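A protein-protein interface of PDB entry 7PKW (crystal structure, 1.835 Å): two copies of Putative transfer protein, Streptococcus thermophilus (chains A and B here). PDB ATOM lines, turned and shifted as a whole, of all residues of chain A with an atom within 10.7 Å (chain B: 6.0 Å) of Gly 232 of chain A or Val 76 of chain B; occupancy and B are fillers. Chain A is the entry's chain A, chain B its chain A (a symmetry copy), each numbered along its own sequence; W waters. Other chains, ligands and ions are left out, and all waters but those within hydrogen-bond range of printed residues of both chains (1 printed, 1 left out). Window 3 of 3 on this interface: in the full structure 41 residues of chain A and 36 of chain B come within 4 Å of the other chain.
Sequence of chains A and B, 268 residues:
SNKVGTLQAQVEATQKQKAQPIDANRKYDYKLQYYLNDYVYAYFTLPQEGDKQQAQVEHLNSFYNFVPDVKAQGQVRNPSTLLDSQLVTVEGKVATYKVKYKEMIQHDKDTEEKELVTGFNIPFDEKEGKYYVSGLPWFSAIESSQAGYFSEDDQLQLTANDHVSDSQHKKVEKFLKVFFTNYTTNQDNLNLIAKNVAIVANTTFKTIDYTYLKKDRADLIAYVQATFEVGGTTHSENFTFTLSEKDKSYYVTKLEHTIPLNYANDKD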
ATOM      1  N   ASN A 202      26.613 -24.009  11.853  1.00  0.00           N
ATOM      2  CA  ASN A 202      26.120 -23.888  13.240  1.00  0.00           C
ATOM      3  C   ASN A 202      24.587 -23.871  13.269  1.00  0.00           C
ATOM      4  O   ASN A 202      24.027 -23.334  14.226  1.00  0.00           O
ATOM      5  CB  ASN A 202      26.689 -22.632  13.923  1.00  0.00           C
ATOM      6  CG  ASN A 202      28.197 -22.672  14.084  1.00  0.00           C
ATOM      7  OD1 ASN A 202      28.722 -23.609  14.686  1.00  0.00           O
ATOM      8  ND2 ASN A 202      28.906 -21.684  13.548  1.00  0.00           N
ATOM      9  N   THR A 203      23.927 -24.476  12.291  1.00  0.00           N
ATOM     10  CA  THR A 203      22.452 -24.412  12.163  1.00  0.00           C
ATOM     11  C   THR A 203      21.825 -25.810  12.226  1.00  0.00           C
ATOM     12  O   THR A 203      22.403 -26.759  11.665  1.00  0.00           O
ATOM     13  CB  THR A 203      22.101 -23.708  10.848  1.00  0.00           C
ATOM     14  OG1 THR A 203      22.721 -22.417  10.908  1.00  0.00           O
ATOM     15  CG2 THR A 203      20.606 -23.571  10.642  1.00  0.00           C
ATOM     16  N   THR A 204      20.657 -25.885  12.849  1.00  0.00           N
ATOM     17  CA  THR A 204      19.698 -26.993  12.763  1.00  0.00           C
ATOM     18  C   THR A 204      18.418 -26.543  12.052  1.00  0.00           C
ATOM     19  O   THR A 204      17.806 -25.509  12.427  1.00  0.00           O
ATOM     20  CB  THR A 204      19.340 -27.581  14.128  1.00  0.00           C
ATOM     21  OG1 THR A 204      20.554 -27.833  14.812  1.00  0.00           O
ATOM     22  CG2 THR A 204      18.598 -28.888  13.965  1.00  0.00           C
ATOM     23  N   LYS A 206      14.589 -26.821  11.481  1.00  0.00           N
ATOM     24  CA  LYS A 206      13.437 -27.245  12.335  1.00  0.00           C
ATOM     25  C   LYS A 206      12.231 -27.562  11.445  1.00  0.00           C
ATOM     26  O   LYS A 206      11.868 -28.750  11.308  1.00  0.00           O
ATOM     27  CB  LYS A 206      13.076 -26.170  13.368  1.00  0.00           C
ATOM     28  CG  LYS A 206      14.219 -25.645  14.243  1.00  0.00           C
ATOM     29  CD  LYS A 206      15.108 -26.713  14.821  1.00  0.00           C
ATOM     30  CE  LYS A 206      14.455 -27.543  15.897  1.00  0.00           C
ATOM     31  NZ  LYS A 206      15.462 -28.237  16.751  1.00  0.00           N
ATOM     32  N   THR A 227      12.053 -22.452   9.499  1.00  0.00           N
ATOM     33  CA  THR A 227      12.616 -22.102  10.807  1.00  0.00           C
ATOM     34  C   THR A 227      13.931 -22.867  10.982  1.00  0.00           C
ATOM     35  O   THR A 227      13.999 -24.067  10.631  1.00  0.00           O
ATOM     36  CB  THR A 227      11.605 -22.361  11.939  1.00  0.00           C
ATOM     37  OG1 THR A 227      10.453 -21.543  11.723  1.00  0.00           O
ATOM     38  CG2 THR A 227      12.197 -22.017  13.287  1.00  0.00           C
ATOM     39  N   PHE A 228      14.917 -22.165  11.502  1.00  0.00           N
ATOM     40  CA  PHE A 228      16.270 -22.663  11.811  1.00  0.00           C
ATOM     41  C   PHE A 228      16.602 -22.289  13.260  1.00  0.00           C
ATOM     42  O   PHE A 228      16.153 -21.247  13.785  1.00  0.00           O
ATOM     43  CB  PHE A 228      17.294 -22.083  10.835  1.00  0.00           C
ATOM     44  CG  PHE A 228      16.984 -22.373   9.394  1.00  0.00           C
ATOM     45  CD1 PHE A 228      17.458 -23.539   8.812  1.00  0.00           C
ATOM     46  CD2 PHE A 228      16.234 -21.483   8.624  1.00  0.00           C
ATOM     47  CE1 PHE A 228      17.161 -23.829   7.485  1.00  0.00           C
ATOM     48  CE2 PHE A 228      15.911 -21.784   7.301  1.00  0.00           C
ATOM     49  CZ  PHE A 228      16.389 -22.958   6.731  1.00  0.00           C
ATOM     50  N   GLU A 229      17.397 -23.135  13.895  1.00  0.00           N
ATOM     51  CA  GLU A 229      17.963 -22.860  15.245  1.00  0.00           C
ATOM     52  C   GLU A 229      19.468 -22.664  15.132  1.00  0.00           C
ATOM     53  O   GLU A 229      20.116 -23.473  14.465  1.00  0.00           O
ATOM     54  CB  GLU A 229      17.654 -24.012  16.199  1.00  0.00           C
ATOM     55  CG  GLU A 229      18.174 -23.736  17.586  1.00  0.00           C
ATOM     56  CD  GLU A 229      17.999 -24.882  18.578  1.00  0.00           C
ATOM     57  OE1 GLU A 229      18.640 -25.934  18.372  1.00  0.00           O
ATOM     58  OE2 GLU A 229      17.272 -24.677  19.564  1.00  0.00           O
ATOM     59  N   VAL A 230      19.980 -21.578  15.699  1.00  0.00           N
ATOM     60  CA  VAL A 230      21.452 -21.255  15.745  1.00  0.00           C
ATOM     61  C   VAL A 230      21.787 -21.036  17.217  1.00  0.00           C
ATOM     62  O   VAL A 230      21.107 -20.200  17.846  1.00  0.00           O
ATOM     63  CB  VAL A 230      21.825 -20.031  14.889  1.00  0.00           C
ATOM     64  CG1 VAL A 230      23.328 -19.710  14.925  1.00  0.00           C
ATOM     65  CG2 VAL A 230      21.383 -20.236  13.439  1.00  0.00           C
ATOM     66  N   GLY A 231      22.666 -21.856  17.782  1.00  0.00           N
ATOM     67  CA  GLY A 231      22.846 -21.900  19.243  1.00  0.00           C
ATOM     68  C   GLY A 231      21.522 -22.210  19.914  1.00  0.00           C
ATOM     69  O   GLY A 231      20.882 -23.238  19.561  1.00  0.00           O
ATOM     70  N   GLY A 232      20.997 -21.290  20.716  1.00  0.00           N
ATOM     71  CA  GLY A 232      19.735 -21.481  21.464  1.00  0.00           C
ATOM     72  C   GLY A 232      18.562 -20.714  20.882  1.00  0.00           C
ATOM     73  O   GLY A 232      17.427 -20.796  21.431  1.00  0.00           O
ATOM     74  N   THR A 233      18.767 -20.065  19.743  1.00  0.00           N
ATOM     75  CA  THR A 233      17.809 -19.082  19.203  1.00  0.00           C
ATOM     76  C   THR A 233      17.244 -19.573  17.867  1.00  0.00           C
ATOM     77  O   THR A 233      18.011 -20.044  17.039  1.00  0.00           O
ATOM     78  CB  THR A 233      18.480 -17.717  19.068  1.00  0.00           C
ATOM     79  OG1 THR A 233      18.813 -17.241  20.373  1.00  0.00           O
ATOM     80  CG2 THR A 233      17.603 -16.716  18.351  1.00  0.00           C
ATOM     81  N   THR A 234      15.946 -19.348  17.644  1.00  0.00           N
ATOM     82  CA  THR A 234      15.293 -19.697  16.375  1.00  0.00           C
ATOM     83  C   THR A 234      15.052 -18.424  15.588  1.00  0.00           C
ATOM     84  O   THR A 234      14.833 -17.323  16.187  1.00  0.00           O
ATOM     85  CB  THR A 234      14.040 -20.566  16.527  1.00  0.00           C
ATOM     86  OG1 THR A 234      12.981 -19.793  17.089  1.00  0.00           O
ATOM     87  CG2 THR A 234      14.283 -21.824  17.332  1.00  0.00           C
ATOM     88  N   HIS A 235      15.089 -18.549  14.260  1.00  0.00           N
ATOM     89  CA  HIS A 235      14.707 -17.462  13.319  1.00  0.00           C
ATOM     90  C   HIS A 235      14.117 -18.071  12.043  1.00  0.00           C
ATOM     91  O   HIS A 235      14.391 -19.248  11.750  1.00  0.00           O
ATOM     92  CB  HIS A 235      15.881 -16.510  13.017  1.00  0.00           C
ATOM     93  CG  HIS A 235      16.899 -17.089  12.096  1.00  0.00           C
ATOM     94  ND1 HIS A 235      17.025 -16.679  10.780  1.00  0.00           N
ATOM     95  CD2 HIS A 235      17.838 -18.032  12.298  1.00  0.00           C
ATOM     96  CE1 HIS A 235      17.978 -17.387  10.212  1.00  0.00           C
ATOM     97  NE2 HIS A 235      18.481 -18.222  11.111  1.00  0.00           N
ATOM     98  N   SER A 236      13.296 -17.289  11.349  1.00  0.00           N
ATOM     99  CA  SER A 236      12.638 -17.695  10.093  1.00  0.00           C
ATOM    100  C   SER A 236      13.360 -17.063   8.919  1.00  0.00           C
ATOM    101  O   SER A 236      13.812 -15.874   9.040  1.00  0.00           O
ATOM    102  CB  SER A 236      11.179 -17.337  10.146  1.00  0.00           C
ATOM    103  OG  SER A 236      10.613 -18.105  11.203  1.00  0.00           O
ATOM    104  N   GLY B  74       5.930 -17.839  17.019  1.00  0.00           N
ATOM    105  CA  GLY B  74       6.967 -16.984  17.628  1.00  0.00           C
ATOM    106  C   GLY B  74       8.316 -17.656  17.567  1.00  0.00           C
ATOM    107  O   GLY B  74       8.372 -18.779  17.056  1.00  0.00           O
ATOM    108  N   GLN B  75       9.357 -17.046  18.121  1.00  0.00           N
ATOM    109  CA  GLN B  75      10.718 -17.653  18.127  1.00  0.00           C
ATOM    110  C   GLN B  75      11.109 -17.922  19.581  1.00  0.00           C
ATOM    111  O   GLN B  75      10.484 -17.329  20.520  1.00  0.00           O
ATOM    112  CB  GLN B  75      11.733 -16.701  17.478  1.00  0.00           C
ATOM    113  CG  GLN B  75      11.329 -16.167  16.119  1.00  0.00           C
ATOM    114  CD  GLN B  75      11.237 -17.218  15.044  1.00  0.00           C
ATOM    115  OE1 GLN B  75      11.767 -18.323  15.185  1.00  0.00           O
ATOM    116  NE2 GLN B  75      10.538 -16.880  13.958  1.00  0.00           N
ATOM    117  N   VAL B  76      12.117 -18.760  19.803  1.00  0.00           N
ATOM    118  CA  VAL B  76      12.854 -18.746  21.083  1.00  0.00           C
ATOM    119  C   VAL B  76      13.988 -17.739  20.906  1.00  0.00           C
ATOM    120  O   VAL B  76      14.859 -17.973  20.015  1.00  0.00           O
ATOM    121  CB  VAL B  76      13.392 -20.151  21.413  1.00  0.00           C
ATOM    122  CG1 VAL B  76      14.090 -20.174  22.756  1.00  0.00           C
ATOM    123  CG2 VAL B  76      12.254 -21.175  21.392  1.00  0.00           C
ATOM    124  N   ARG B  77      14.005 -16.772  21.821  1.00  0.00           N
ATOM    125  CA  ARG B  77      14.919 -15.611  21.872  1.00  0.00           C
ATOM    126  C   ARG B  77      15.717 -15.712  23.174  1.00  0.00           C
ATOM    127  O   ARG B  77      15.076 -16.077  24.185  1.00  0.00           O
ATOM    128  CB  ARG B  77      14.075 -14.331  21.825  1.00  0.00           C
ATOM    129  CG  ARG B  77      13.187 -14.226  20.594  1.00  0.00           C
ATOM    130  CD  ARG B  77      14.064 -14.565  19.410  1.00  0.00           C
ATOM    131  NE  ARG B  77      15.266 -13.764  19.488  1.00  0.00           N
ATOM    132  CZ  ARG B  77      15.321 -12.466  19.230  1.00  0.00           C
ATOM    133  NH1 ARG B  77      14.189 -11.810  18.990  1.00  0.00           N
ATOM    134  NH2 ARG B  77      16.500 -11.835  19.302  1.00  0.00           N
ATOM    135  N   ASN B  78      17.048 -15.560  23.122  1.00  0.00           N
ATOM    136  CA  ASN B  78      17.890 -15.470  24.336  1.00  0.00           C
ATOM    137  C   ASN B  78      18.600 -14.127  24.319  1.00  0.00           C
ATOM    138  O   ASN B  78      18.867 -13.559  23.234  1.00  0.00           O
ATOM    139  CB  ASN B  78      18.921 -16.602  24.366  1.00  0.00           C
ATOM    140  CG  ASN B  78      18.260 -17.947  24.562  1.00  0.00           C
ATOM    141  OD1 ASN B  78      17.642 -18.160  25.570  1.00  0.00           O
ATOM    142  ND2 ASN B  78      18.254 -18.784  23.550  1.00  0.00           N
ATOM    143  N   GLU B 103      25.549 -15.230  23.070  1.00  0.00           N
ATOM    144  CA  GLU B 103      24.159 -15.512  23.481  1.00  0.00           C
ATOM    145  C   GLU B 103      24.219 -16.117  24.884  1.00  0.00           C
ATOM    146  O   GLU B 103      25.035 -17.033  25.087  1.00  0.00           O
ATOM    147  CB  GLU B 103      23.522 -16.442  22.455  1.00  0.00           C
ATOM    148  CG  GLU B 103      22.452 -17.339  23.024  1.00  0.00           C
ATOM    149  CD  GLU B 103      21.794 -18.266  22.018  1.00  0.00           C
ATOM    150  OE1 GLU B 103      22.513 -19.106  21.419  1.00  0.00           O
ATOM    151  OE2 GLU B 103      20.542 -18.169  21.870  1.00  0.00           O
ATOM    152  N   ILE B 105      22.354 -18.299  27.443  1.00  0.00           N
ATOM    153  CA  ILE B 105      21.300 -19.352  27.578  1.00  0.00           C
ATOM    154  C   ILE B 105      21.113 -19.671  29.073  1.00  0.00           C
ATOM    155  O   ILE B 105      22.103 -20.072  29.709  1.00  0.00           O
ATOM    156  CB  ILE B 105      21.641 -20.613  26.762  1.00  0.00           C
ATOM    157  CG1 ILE B 105      21.936 -20.294  25.292  1.00  0.00           C
ATOM    158  CG2 ILE B 105      20.503 -21.626  26.883  1.00  0.00           C
ATOM    159  CD1 ILE B 105      23.183 -20.945  24.761  1.00  0.00           C
ATOM    160  N   LEU B 116      29.486 -16.985  19.124  1.00  0.00           N
ATOM    161  CA  LEU B 116      29.087 -17.550  17.835  1.00  0.00           C
ATOM    162  C   LEU B 116      29.517 -16.575  16.746  1.00  0.00           C
ATOM    163  O   LEU B 116      29.612 -15.361  17.004  1.00  0.00           O
ATOM    164  CB  LEU B 116      27.568 -17.729  17.843  1.00  0.00           C
ATOM    165  CG  LEU B 116      27.056 -18.955  18.604  1.00  0.00           C
ATOM    166  CD1 LEU B 116      25.808 -18.605  19.390  1.00  0.00           C
ATOM    167  CD2 LEU B 116      26.793 -20.116  17.645  1.00  0.00           C
HETATM  168  O   HOH W   1      17.506 -21.646  23.954  1.00  0.00           O
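Among the printed residues, pairs that only touch across the chains: Val 230 of chain A with Glu 103 of chain B (3.99 Å), Gly 231 of chain A with Glu 103 of chain B (3.6 Å), Gly 232 of chain A with Val 76 of chain B (3.6 Å), Thr 233 of chain A with Val 76 of chain B (3.3 Å), Thr 233 of chain A with Arg 77 of chain B (3.9 Å) and Thr 233 of chain A with Asn 78 of chain B (3.6 Å).
The side-chain hydroxyl of Ser 236 of chain A lies within hydrogen-bond range of the side-chain hydroxyl of Thr 227 of chain A (3.5 Å).
O of Phe 228 of chain A is in hydrogen-bond range of N of His 235 of chain A (2.9 Å).
ND2 of Asn 78 of chain B sits at hydrogen-bond distance from OE2 of Glu 103 of chain B (2.9 Å).
O of Gly 232 of chain A sits at hydrogen-bond distance from ND2 of Asn 78 of chain B, at 3.0 Å.
N of Gly 232 of chain A sits at hydrogen-bond distance from OE1 of Glu 103 of chain B (2.7 Å).
The side-chain carboxylate (OE2) of Glu 103 of chain B lies within hydrogen-bond range of the side-chain hydroxyl (OG1) of Thr 233 of chain A (2.5 Å).
The side-chain hydroxyl of Thr 234 of chain A is in hydrogen-bond range of the side-chain amide oxygen of Gln 75 of chain B (2.7 Å).
The backbone carbonyl oxygen of Val 76 of chain B sits at hydrogen-bond distance from the backbone NH of Thr 234 of chain A.
The backbone NH of His 235 of chain A sits at hydrogen-bond distance from the side-chain amide oxygen of Gln 75 of chain B (3.5 Å).
The side-chain hydroxyl (OG) of Ser 236 of chain A lies within hydrogen-bond range of the side-chain amide nitrogen (NE2) of Gln 75 of chain B.
Water W1 bridges O of Gly 232 of chain A (2.7 Å) and ND2 of Asn 78 of chain B (3.0 Å).
Thr 227 of chain A touches none of the printed residues of chain B.
Printed residues of chain B within 4 Å of Gly 231 of chain A: Glu 103 (3.6 Å).
Val 76 of chain B touches three residues of chain A.
Printed residues of chain A within 4 Å of Glu 103 of chain B: Val 230, Gly 231, Gly 232 and Thr 233.
Hydrophobic or aromatic side chains of chain B that line the printed part of chain A: Val 76.
Among the printed residues, no Asp or Glu carboxylate lies within 4 Å of a Lys or Arg side-chain nitrogen of the other chain.
No position is printed for both chains.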
